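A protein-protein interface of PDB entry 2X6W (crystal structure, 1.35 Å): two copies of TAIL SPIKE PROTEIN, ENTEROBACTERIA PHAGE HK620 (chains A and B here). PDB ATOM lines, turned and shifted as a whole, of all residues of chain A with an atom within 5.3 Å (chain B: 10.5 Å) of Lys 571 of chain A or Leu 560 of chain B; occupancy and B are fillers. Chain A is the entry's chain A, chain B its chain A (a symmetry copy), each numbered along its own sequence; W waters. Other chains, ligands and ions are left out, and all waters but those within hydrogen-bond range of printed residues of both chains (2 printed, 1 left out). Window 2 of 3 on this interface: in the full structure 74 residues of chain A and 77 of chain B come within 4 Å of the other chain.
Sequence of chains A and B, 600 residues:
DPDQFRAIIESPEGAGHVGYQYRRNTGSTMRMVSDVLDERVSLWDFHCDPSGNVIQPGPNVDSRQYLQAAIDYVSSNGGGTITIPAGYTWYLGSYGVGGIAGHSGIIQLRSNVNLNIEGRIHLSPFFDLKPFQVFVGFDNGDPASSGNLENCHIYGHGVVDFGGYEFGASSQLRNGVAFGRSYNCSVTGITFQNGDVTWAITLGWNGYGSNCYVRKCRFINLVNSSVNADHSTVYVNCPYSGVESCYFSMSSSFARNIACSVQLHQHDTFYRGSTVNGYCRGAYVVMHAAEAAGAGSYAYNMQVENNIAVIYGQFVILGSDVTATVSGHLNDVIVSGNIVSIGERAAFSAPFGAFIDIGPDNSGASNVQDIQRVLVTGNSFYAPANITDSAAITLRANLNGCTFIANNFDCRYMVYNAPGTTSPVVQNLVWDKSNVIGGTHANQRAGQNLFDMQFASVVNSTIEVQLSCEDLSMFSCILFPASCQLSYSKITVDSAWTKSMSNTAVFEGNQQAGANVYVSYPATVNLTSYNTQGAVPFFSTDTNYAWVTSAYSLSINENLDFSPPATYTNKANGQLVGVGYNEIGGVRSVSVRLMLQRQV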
ATOM      1  N   PHE A 539     -29.509 -36.219  30.280  1.00  0.00           N
ATOM      2  CA  PHE A 539     -28.669 -36.130  29.102  1.00  0.00           C
ATOM      3  C   PHE A 539     -29.375 -36.839  27.943  1.00  0.00           C
ATOM      4  O   PHE A 539     -29.994 -37.889  28.133  1.00  0.00           O
ATOM      5  CB  PHE A 539     -27.326 -36.864  29.280  1.00  0.00           C
ATOM      6  CG  PHE A 539     -26.490 -36.354  30.421  1.00  0.00           C
ATOM      7  CD1 PHE A 539     -26.606 -36.944  31.675  1.00  0.00           C
ATOM      8  CD2 PHE A 539     -25.599 -35.331  30.239  1.00  0.00           C
ATOM      9  CE1 PHE A 539     -25.861 -36.483  32.719  1.00  0.00           C
ATOM     10  CE2 PHE A 539     -24.836 -34.859  31.285  1.00  0.00           C
ATOM     11  CZ  PHE A 539     -24.964 -35.437  32.527  1.00  0.00           C
ATOM     12  N   ALA A 546     -24.880 -30.829  18.831  1.00  0.00           N
ATOM     13  CA  ALA A 546     -23.740 -29.917  19.076  1.00  0.00           C
ATOM     14  C   ALA A 546     -24.004 -28.475  18.665  1.00  0.00           C
ATOM     15  O   ALA A 546     -23.326 -27.565  19.152  1.00  0.00           O
ATOM     16  CB  ALA A 546     -22.442 -30.417  18.406  1.00  0.00           C
ATOM     17  N   THR A 569     -29.171 -27.129  27.708  1.00  0.00           N
ATOM     18  CA  THR A 569     -28.109 -26.648  26.837  1.00  0.00           C
ATOM     19  C   THR A 569     -27.422 -27.871  26.247  1.00  0.00           C
ATOM     20  O   THR A 569     -27.963 -28.965  26.338  1.00  0.00           O
ATOM     21  CB  THR A 569     -27.057 -25.806  27.655  1.00  0.00           C
ATOM     22  OG1 THR A 569     -26.696 -26.544  28.834  1.00  0.00           O
ATOM     23  CG2 THR A 569     -27.582 -24.447  28.049  1.00  0.00           C
ATOM     24  N   ASN A 570     -26.301 -27.695  25.583  1.00  0.00           N
ATOM     25  CA  ASN A 570     -25.559 -28.801  25.071  1.00  0.00           C
ATOM     26  C   ASN A 570     -24.191 -29.007  25.689  1.00  0.00           C
ATOM     27  O   ASN A 570     -23.791 -28.289  26.611  1.00  0.00           O
ATOM     28  CB  ASN A 570     -25.529 -28.728  23.572  1.00  0.00           C
ATOM     29  CG  ASN A 570     -24.601 -27.696  23.027  1.00  0.00           C
ATOM     30  OD1 ASN A 570     -24.103 -26.770  23.716  1.00  0.00           O
ATOM     31  ND2 ASN A 570     -24.368 -27.816  21.716  1.00  0.00           N
ATOM     32  N   LYS A 571     -23.501 -30.031  25.186  1.00  0.00           N
ATOM     33  CA  LYS A 571     -22.150 -30.411  25.589  1.00  0.00           C
ATOM     34  C   LYS A 571     -21.359 -30.622  24.308  1.00  0.00           C
ATOM     35  O   LYS A 571     -21.916 -30.833  23.234  1.00  0.00           O
ATOM     36  CB  LYS A 571     -22.163 -31.761  26.336  1.00  0.00           C
ATOM     37  CG  LYS A 571     -22.724 -31.754  27.725  1.00  0.00           C
ATOM     38  CD  LYS A 571     -22.917 -33.183  28.256  1.00  0.00           C
ATOM     39  CE  LYS A 571     -21.686 -34.071  28.207  1.00  0.00           C
ATOM     40  NZ  LYS A 571     -21.928 -35.417  28.871  1.00  0.00           N
ATOM     41  N   ALA A 572     -20.048 -30.657  24.446  1.00  0.00           N
ATOM     42  CA  ALA A 572     -19.130 -30.753  23.302  1.00  0.00           C
ATOM     43  C   ALA A 572     -19.349 -31.979  22.454  1.00  0.00           C
ATOM     44  O   ALA A 572     -19.070 -31.956  21.259  1.00  0.00           O
ATOM     45  CB  ALA A 572     -17.681 -30.789  23.774  1.00  0.00           C
ATOM     46  N   ASN A 573     -19.809 -33.060  23.075  1.00  0.00           N
ATOM     47  CA  ASN A 573     -19.996 -34.326  22.370  1.00  0.00           C
ATOM     48  C   ASN A 573     -21.318 -34.402  21.635  1.00  0.00           C
ATOM     49  O   ASN A 573     -21.647 -35.426  21.055  1.00  0.00           O
ATOM     50  CB  ASN A 573     -19.869 -35.510  23.344  1.00  0.00           C
ATOM     51  CG  ASN A 573     -21.002 -35.557  24.364  1.00  0.00           C
ATOM     52  OD1 ASN A 573     -21.787 -34.636  24.459  1.00  0.00           O
ATOM     53  ND2 ASN A 573     -21.054 -36.629  25.140  1.00  0.00           N
ATOM     54  N   GLY A 574     -22.100 -33.329  21.679  1.00  0.00           N
ATOM     55  CA  GLY A 574     -23.365 -33.268  20.971  1.00  0.00           C
ATOM     56  C   GLY A 574     -24.584 -33.697  21.770  1.00  0.00           C
ATOM     57  O   GLY A 574     -25.725 -33.683  21.239  1.00  0.00           O
ATOM     58  N   GLN A 575     -24.397 -34.062  23.042  1.00  0.00           N
ATOM     59  CA  GLN A 575     -25.559 -34.349  23.906  1.00  0.00           C
ATOM     60  C   GLN A 575     -26.208 -33.039  24.373  1.00  0.00           C
ATOM     61  O   GLN A 575     -25.537 -32.020  24.540  1.00  0.00           O
ATOM     62  CB  GLN A 575     -25.144 -35.133  25.144  1.00  0.00           C
ATOM     63  CG  GLN A 575     -24.770 -36.565  24.926  1.00  0.00           C
ATOM     64  CD  GLN A 575     -24.411 -37.218  26.254  1.00  0.00           C
ATOM     65  OE1 GLN A 575     -23.382 -36.905  26.846  1.00  0.00           O
ATOM     66  NE2 GLN A 575     -25.279 -38.086  26.751  1.00  0.00           N
ATOM     67  N   LEU A 576     -27.515 -33.084  24.579  1.00  0.00           N
ATOM     68  CA  LEU A 576     -28.209 -32.097  25.389  1.00  0.00           C
ATOM     69  C   LEU A 576     -28.042 -32.497  26.855  1.00  0.00           C
ATOM     70  O   LEU A 576     -27.964 -33.676  27.189  1.00  0.00           O
ATOM     71  CB  LEU A 576     -29.683 -32.060  25.018  1.00  0.00           C
ATOM     72  CG  LEU A 576     -30.028 -31.572  23.616  1.00  0.00           C
ATOM     73  CD1 LEU A 576     -31.560 -31.651  23.445  1.00  0.00           C
ATOM     74  CD2 LEU A 576     -29.529 -30.170  23.390  1.00  0.00           C
ATOM     75  N   VAL A 577     -28.047 -31.485  27.721  1.00  0.00           N
ATOM     76  CA  VAL A 577     -27.979 -31.626  29.174  1.00  0.00           C
ATOM     77  C   VAL A 577     -28.859 -30.584  29.854  1.00  0.00           C
ATOM     78  O   VAL A 577     -28.887 -29.437  29.453  1.00  0.00           O
ATOM     79  CB  VAL A 577     -26.529 -31.538  29.701  1.00  0.00           C
ATOM     80  CG1 VAL A 577     -25.849 -30.255  29.295  1.00  0.00           C
ATOM     81  CG2 VAL A 577     -26.474 -31.753  31.233  1.00  0.00           C
ATOM     82  N   GLN B 533     -18.926 -29.938  42.524  1.00  0.00           N
ATOM     83  CA  GLN B 533     -19.320 -30.953  41.567  1.00  0.00           C
ATOM     84  C   GLN B 533     -20.836 -31.107  41.627  1.00  0.00           C
ATOM     85  O   GLN B 533     -21.429 -31.001  42.688  1.00  0.00           O
ATOM     86  CB  GLN B 533     -18.615 -32.295  41.840  1.00  0.00           C
ATOM     87  CG  GLN B 533     -18.777 -33.339  40.747  1.00  0.00           C
ATOM     88  CD  GLN B 533     -20.090 -34.092  40.804  1.00  0.00           C
ATOM     89  OE1 GLN B 533     -20.704 -34.237  41.875  1.00  0.00           O
ATOM     90  NE2 GLN B 533     -20.511 -34.620  39.657  1.00  0.00           N
ATOM     91  N   SER B 553     -29.680 -18.787  27.201  1.00  0.00           N
ATOM     92  CA  SER B 553     -28.512 -18.955  26.341  1.00  0.00           C
ATOM     93  C   SER B 553     -28.805 -18.844  24.859  1.00  0.00           C
ATOM     94  O   SER B 553     -29.731 -19.502  24.360  1.00  0.00           O
ATOM     95  CB  SER B 553     -27.933 -20.347  26.572  1.00  0.00           C
ATOM     96  OG  SER B 553     -26.786 -20.539  25.763  1.00  0.00           O
ATOM     97  N   SER B 555     -25.809 -19.186  23.013  1.00  0.00           N
ATOM     98  CA  SER B 555     -24.483 -19.704  22.676  1.00  0.00           C
ATOM     99  C   SER B 555     -24.408 -21.195  22.856  1.00  0.00           C
ATOM    100  O   SER B 555     -25.066 -21.726  23.756  1.00  0.00           O
ATOM    101  CB  SER B 555     -23.418 -19.238  23.652  1.00  0.00           C
ATOM    102  OG  SER B 555     -23.293 -17.892  23.694  1.00  0.00           O
ATOM    103  N   ILE B 556     -23.544 -21.862  22.075  1.00  0.00           N
ATOM    104  CA  ILE B 556     -23.289 -23.266  22.354  1.00  0.00           C
ATOM    105  C   ILE B 556     -22.255 -23.400  23.452  1.00  0.00           C
ATOM    106  O   ILE B 556     -21.553 -22.455  23.798  1.00  0.00           O
ATOM    107  CB  ILE B 556     -22.837 -24.074  21.107  1.00  0.00           C
ATOM    108  CG1 ILE B 556     -21.497 -23.562  20.588  1.00  0.00           C
ATOM    109  CG2 ILE B 556     -23.912 -24.122  20.022  1.00  0.00           C
ATOM    110  CD1 ILE B 556     -20.859 -24.574  19.581  1.00  0.00           C
ATOM    111  N   ASN B 557     -22.205 -24.588  24.015  1.00  0.00           N
ATOM    112  CA  ASN B 557     -21.255 -24.942  25.062  1.00  0.00           C
ATOM    113  C   ASN B 557     -20.199 -25.879  24.477  1.00  0.00           C
ATOM    114  O   ASN B 557     -20.495 -27.048  24.173  1.00  0.00           O
ATOM    115  CB  ASN B 557     -21.996 -25.626  26.206  1.00  0.00           C
ATOM    116  CG  ASN B 557     -21.071 -26.147  27.271  1.00  0.00           C
ATOM    117  OD1 ASN B 557     -20.050 -25.528  27.553  1.00  0.00           O
ATOM    118  ND2 ASN B 557     -21.415 -27.282  27.874  1.00  0.00           N
ATOM    119  N   GLU B 558     -18.977 -25.367  24.338  1.00  0.00           N
ATOM    120  CA  GLU B 558     -17.855 -26.132  23.760  1.00  0.00           C
ATOM    121  C   GLU B 558     -17.244 -27.167  24.721  1.00  0.00           C
ATOM    122  O   GLU B 558     -16.387 -27.966  24.324  1.00  0.00           O
ATOM    123  CB  GLU B 558     -16.720 -25.173  23.271  1.00  0.00           C
ATOM    124  CG  GLU B 558     -15.938 -24.549  24.452  1.00  0.00           C
ATOM    125  CD  GLU B 558     -14.723 -23.716  24.102  1.00  0.00           C
ATOM    126  OE1 GLU B 558     -14.167 -23.841  22.977  1.00  0.00           O
ATOM    127  OE2 GLU B 558     -14.316 -22.949  25.011  1.00  0.00           O
ATOM    128  N   ASN B 559     -17.682 -27.161  25.966  1.00  0.00           N
ATOM    129  CA  ASN B 559     -17.128 -27.973  27.039  1.00  0.00           C
ATOM    130  C   ASN B 559     -17.775 -29.322  27.132  1.00  0.00           C
ATOM    131  O   ASN B 559     -18.972 -29.469  26.862  1.00  0.00           O
ATOM    132  CB  ASN B 559     -17.282 -27.229  28.362  1.00  0.00           C
ATOM    133  CG  ASN B 559     -16.533 -25.927  28.332  1.00  0.00           C
ATOM    134  OD1 ASN B 559     -15.304 -25.912  28.418  1.00  0.00           O
ATOM    135  ND2 ASN B 559     -17.248 -24.833  28.107  1.00  0.00           N
ATOM    136  N   LEU B 560     -16.989 -30.304  27.582  1.00  0.00           N
ATOM    137  CA  LEU B 560     -17.494 -31.624  27.936  1.00  0.00           C
ATOM    138  C   LEU B 560     -17.775 -31.751  29.440  1.00  0.00           C
ATOM    139  O   LEU B 560     -18.766 -32.340  29.838  1.00  0.00           O
ATOM    140  CB  LEU B 560     -16.533 -32.742  27.465  1.00  0.00           C
ATOM    141  CG  LEU B 560     -17.115 -34.156  27.499  1.00  0.00           C
ATOM    142  CD1 LEU B 560     -18.253 -34.296  26.484  1.00  0.00           C
ATOM    143  CD2 LEU B 560     -16.028 -35.191  27.210  1.00  0.00           C
ATOM    144  N   ASP B 561     -16.881 -31.195  30.255  1.00  0.00           N
ATOM    145  CA  ASP B 561     -16.864 -31.466  31.682  1.00  0.00           C
ATOM    146  C   ASP B 561     -17.891 -30.676  32.491  1.00  0.00           C
ATOM    147  O   ASP B 561     -18.061 -30.937  33.683  1.00  0.00           O
ATOM    148  CB  ASP B 561     -15.471 -31.202  32.266  1.00  0.00           C
ATOM    149  CG  ASP B 561     -14.398 -32.146  31.749  1.00  0.00           C
ATOM    150  OD1 ASP B 561     -14.687 -33.114  31.008  1.00  0.00           O
ATOM    151  OD2 ASP B 561     -13.241 -31.871  32.136  1.00  0.00           O
ATOM    152  N   PHE B 562     -18.522 -29.684  31.872  1.00  0.00           N
ATOM    153  CA  PHE B 562     -19.546 -28.908  32.531  1.00  0.00           C
ATOM    154  C   PHE B 562     -20.434 -28.262  31.505  1.00  0.00           C
ATOM    155  O   PHE B 562     -20.105 -28.238  30.308  1.00  0.00           O
ATOM    156  CB  PHE B 562     -18.960 -27.831  33.445  1.00  0.00           C
ATOM    157  CG  PHE B 562     -18.347 -26.677  32.725  1.00  0.00           C
ATOM    158  CD1 PHE B 562     -17.031 -26.717  32.303  1.00  0.00           C
ATOM    159  CD2 PHE B 562     -19.081 -25.538  32.483  1.00  0.00           C
ATOM    160  CE1 PHE B 562     -16.486 -25.605  31.653  1.00  0.00           C
ATOM    161  CE2 PHE B 562     -18.546 -24.449  31.860  1.00  0.00           C
ATOM    162  CZ  PHE B 562     -17.249 -24.470  31.432  1.00  0.00           C
ATOM    163  N   SER B 563     -21.544 -27.703  31.993  1.00  0.00           N
ATOM    164  CA  SER B 563     -22.400 -26.885  31.169  1.00  0.00           C
ATOM    165  C   SER B 563     -22.878 -25.701  32.032  1.00  0.00           C
ATOM    166  O   SER B 563     -23.213 -25.874  33.218  1.00  0.00           O
ATOM    167  CB  SER B 563     -23.581 -27.699  30.632  1.00  0.00           C
ATOM    168  OG  SER B 563     -24.302 -28.327  31.680  1.00  0.00           O
ATOM    169  N   PRO B 564     -22.908 -24.480  31.447  1.00  0.00           N
ATOM    170  CA  PRO B 564     -23.527 -23.369  32.128  1.00  0.00           C
ATOM    171  C   PRO B 564     -25.042 -23.552  32.103  1.00  0.00           C
ATOM    172  O   PRO B 564     -25.555 -24.412  31.407  1.00  0.00           O
ATOM    173  CB  PRO B 564     -23.089 -22.160  31.278  1.00  0.00           C
ATOM    174  CG  PRO B 564     -23.041 -22.731  29.859  1.00  0.00           C
ATOM    175  CD  PRO B 564     -22.494 -24.140  30.063  1.00  0.00           C
ATOM    176  N   ALA B 566     -28.893 -23.099  31.150  1.00  0.00           N
ATOM    177  CA  ALA B 566     -29.658 -22.700  29.988  1.00  0.00           C
ATOM    178  C   ALA B 566     -30.374 -21.380  30.234  1.00  0.00           C
ATOM    179  O   ALA B 566     -30.555 -20.592  29.314  1.00  0.00           O
ATOM    180  CB  ALA B 566     -30.644 -23.783  29.562  1.00  0.00           C
ATOM    181  N   GLY B 580     -26.215 -24.546  36.628  1.00  0.00           N
ATOM    182  CA  GLY B 580     -25.604 -25.401  35.615  1.00  0.00           C
ATOM    183  C   GLY B 580     -25.170 -26.709  36.228  1.00  0.00           C
ATOM    184  O   GLY B 580     -25.632 -27.116  37.290  1.00  0.00           O
ATOM    185  N   TYR B 581     -24.286 -27.416  35.532  1.00  0.00           N
ATOM    186  CA  TYR B 581     -23.883 -28.753  35.960  1.00  0.00           C
ATOM    187  C   TYR B 581     -22.386 -28.984  35.745  1.00  0.00           C
ATOM    188  O   TYR B 581     -21.895 -28.866  34.630  1.00  0.00           O
ATOM    189  CB  TYR B 581     -24.723 -29.854  35.271  1.00  0.00           C
ATOM    190  CG  TYR B 581     -24.503 -31.195  35.950  1.00  0.00           C
ATOM    191  CD1 TYR B 581     -25.095 -31.456  37.181  1.00  0.00           C
ATOM    192  CD2 TYR B 581     -23.639 -32.148  35.407  1.00  0.00           C
ATOM    193  CE1 TYR B 581     -24.860 -32.644  37.857  1.00  0.00           C
ATOM    194  CE2 TYR B 581     -23.398 -33.357  36.066  1.00  0.00           C
ATOM    195  CZ  TYR B 581     -24.007 -33.581  37.305  1.00  0.00           C
ATOM    196  OH  TYR B 581     -23.775 -34.759  38.006  1.00  0.00           O
ATOM    197  N   ASN B 582     -21.682 -29.280  36.834  1.00  0.00           N
ATOM    198  CA  ASN B 582     -20.287 -29.636  36.812  1.00  0.00           C
ATOM    199  C   ASN B 582     -20.155 -31.184  36.859  1.00  0.00           C
ATOM    200  O   ASN B 582     -20.326 -31.805  37.922  1.00  0.00           O
ATOM    201  CB  ASN B 582     -19.566 -29.067  38.051  1.00  0.00           C
ATOM    202  CG  ASN B 582     -18.658 -27.864  37.763  1.00  0.00           C
ATOM    203  OD1 ASN B 582     -18.257 -27.609  36.616  1.00  0.00           O
ATOM    204  ND2 ASN B 582     -18.298 -27.153  38.841  1.00  0.00           N
ATOM    205  N   GLU B 583     -19.861 -31.828  35.726  1.00  0.00           N
ATOM    206  CA  GLU B 583     -19.629 -33.268  35.757  1.00  0.00           C
ATOM    207  C   GLU B 583     -18.440 -33.577  36.655  1.00  0.00           C
ATOM    208  O   GLU B 583     -18.469 -34.536  37.447  1.00  0.00           O
ATOM    209  CB  GLU B 583     -19.404 -33.836  34.341  1.00  0.00           C
ATOM    210  CG  GLU B 583     -19.056 -35.331  34.240  1.00  0.00           C
ATOM    211  CD  GLU B 583     -20.222 -36.239  34.570  1.00  0.00           C
ATOM    212  OE1 GLU B 583     -21.354 -35.844  34.248  1.00  0.00           O
ATOM    213  OE2 GLU B 583     -20.009 -37.357  35.113  1.00  0.00           O
ATOM    214  N   ILE B 584     -17.410 -32.740  36.519  1.00  0.00           N
ATOM    215  CA  ILE B 584     -16.250 -32.717  37.405  1.00  0.00           C
ATOM    216  C   ILE B 584     -16.248 -31.335  38.033  1.00  0.00           C
ATOM    217  O   ILE B 584     -16.641 -30.362  37.387  1.00  0.00           O
ATOM    218  CB  ILE B 584     -14.914 -32.937  36.643  1.00  0.00           C
ATOM    219  CG1 ILE B 584     -14.969 -34.299  35.948  1.00  0.00           C
ATOM    220  CG2 ILE B 584     -13.706 -32.825  37.604  1.00  0.00           C
ATOM    221  CD1 ILE B 584     -13.787 -34.533  35.012  1.00  0.00           C
ATOM    222  N   GLY B 585     -15.873 -31.258  39.309  1.00  0.00           N
ATOM    223  CA  GLY B 585     -15.785 -29.973  39.999  1.00  0.00           C
ATOM    224  C   GLY B 585     -14.741 -29.048  39.408  1.00  0.00           C
ATOM    225  O   GLY B 585     -13.877 -29.442  38.607  1.00  0.00           O
ATOM    226  N   ARG B 588     -15.621 -22.438  37.172  1.00  0.00           N
ATOM    227  CA  ARG B 588     -15.702 -22.213  35.731  1.00  0.00           C
ATOM    228  C   ARG B 588     -15.852 -20.730  35.435  1.00  0.00           C
ATOM    229  O   ARG B 588     -16.412 -19.991  36.241  1.00  0.00           O
ATOM    230  CB  ARG B 588     -16.886 -22.976  35.138  1.00  0.00           C
ATOM    231  CG  ARG B 588     -16.974 -24.434  35.500  1.00  0.00           C
ATOM    232  CD  ARG B 588     -15.723 -25.215  35.167  1.00  0.00           C
ATOM    233  NE  ARG B 588     -15.902 -26.634  35.473  1.00  0.00           N
ATOM    234  CZ  ARG B 588     -15.087 -27.587  35.028  1.00  0.00           C
ATOM    235  NH1 ARG B 588     -14.020 -27.287  34.283  1.00  0.00           N
ATOM    236  NH2 ARG B 588     -15.326 -28.861  35.311  1.00  0.00           N
ATOM    237  N   VAL B 590     -16.936 -18.409  31.944  1.00  0.00           N
ATOM    238  CA  VAL B 590     -17.399 -18.411  30.562  1.00  0.00           C
ATOM    239  C   VAL B 590     -17.943 -17.028  30.167  1.00  0.00           C
ATOM    240  O   VAL B 590     -18.389 -16.264  31.020  1.00  0.00           O
ATOM    241  CB  VAL B 590     -18.535 -19.483  30.355  1.00  0.00           C
ATOM    242  CG1 VAL B 590     -18.001 -20.901  30.611  1.00  0.00           C
ATOM    243  CG2 VAL B 590     -19.732 -19.197  31.210  1.00  0.00           C
HETATM  244  O   HOH W   1     -21.369 -34.680  31.572  1.00  0.00           O
HETATM  245  O   HOH W   2     -26.017 -24.835  24.544  1.00  0.00           O
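No position is printed for both chains. Of the 15 pairs that touch across the chains among the printed residues, none has its exchanged pair printed and touching as well.
Water W2 lies within hydrogen-bond range of OD1 of Asn 570 of chain A (2.8 Å) and O of Ser 555 of chain B (3.3 Å). Water W1 bridges NZ of Lys 571 of chain A (2.9 Å) and OE1 of Glu 583 of chain B (2.9 Å).
Leu 560 of chain B touches just these residues of chain A: Lys 571, Ala 572 and Asn 573. Of chain B, only Ile 556 (3.6 Å) comes within 4 Å of Ala 546 of chain A. Of the printed residues of chain B, Ala 572 of chain A touches Asn 557 (3.6 Å), Glu 558 (3.2 Å), Asn 559 (2.9 Å) and Leu 560 (3.9 Å). Of chain B, only Leu 560 comes within 4 Å of Asn 573 of chain A. No residue of chain B comes within 4 Å of Gly 574 of chain A. Printed residues of chain A within 4 Å of Asn 557 of chain B: Asn 570, Lys 571 and Ala 572. Of the printed residues of chain B, Thr 569 of chain A touches Ser 563 (3.8 Å), Pro 564 (3.5 Å) and Ala 566 (3.3 Å). Of the printed residues of chain A, Pro 564 of chain B touches Thr 569 (3.5 Å). Of the printed residues of chain B, Val 577 of chain A touches Ser 563. Of the printed residues of chain A, Ile 556 of chain B touches Ala 546 and Asn 570. Asn 582 of chain B touches none of the printed residues of chain A. The nearest printed residue of chain B that does not touch Lys 571 of chain A is Ser 563 of chain B (5.1 Å). The nearest printed residue of chain A that does not touch Leu 560 of chain B is Gln 575 of chain A (5.8 Å).
The backbone NH of Ala 572 of chain A sits at hydrogen-bond distance from the backbone carbonyl oxygen of Asn 559 of chain B (2.9 Å). The side-chain amide nitrogen (ND2) of Asn 557 of chain B lies within hydrogen-bond range of the backbone carbonyl oxygen (O) of Asn 570 of chain A (2.9 Å).
Ser 563 of chain B touches Thr 569 of chain A. O of Pro 564 of chain B touches OG1 of Thr 569 of chain A (3.5 Å). Ala 566 of chain B touches Thr 569 of chain A (CA to CG2, 3.3 Å). Asn 557 of chain B touches Lys 571 of chain A. Asn 559 of chain B touches Lys 571 of chain A. O of Leu 560 of chain B touches CE of Lys 571 of chain A, at 3.8 Å. Ala 572 of chain A touches Asn 557 of chain B. Ala 572 of chain A touches Glu 558 of chain B (CB to O, 3.2 Å). CG of Asn 573 of chain A touches CD1 of Leu 560 of chain B (3.7 Å). OG of Ser 563 of chain B touches CG1 of Val 577 of chain A (3.4 Å).
NZ of Lys 571 of chain A sits at hydrogen-bond distance from OE1 of Gln 575 of chain A (2.9 Å). The side-chain amide nitrogen (ND2) of Asn 573 of chain A sits at hydrogen-bond distance from the side-chain amide oxygen (OE1) of Gln 575 of chain A. The side-chain amide nitrogen of Asn 559 of chain B is in hydrogen-bond range of the side-chain amide oxygen of Asn 557 of chain B (2.9 Å). N of Ser 563 of chain B is in hydrogen-bond range of O of Tyr 581 of chain B (2.9 Å). The backbone carbonyl oxygen of Ala 566 of chain B lies within hydrogen-bond range of the backbone NH of Ser 553 of chain B. The backbone carbonyl oxygen of Ala 546 of chain A lies within hydrogen-bond range of the side-chain amide nitrogen of Asn 570 of chain A (2.8 Å).
Of the 11 printed residues of chain A, 7 touch a printed residue of chain B. Hydrophobic or aromatic side chains of chain B that line the printed part of chain A: Ile 556, Leu 560 and Ala 566.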
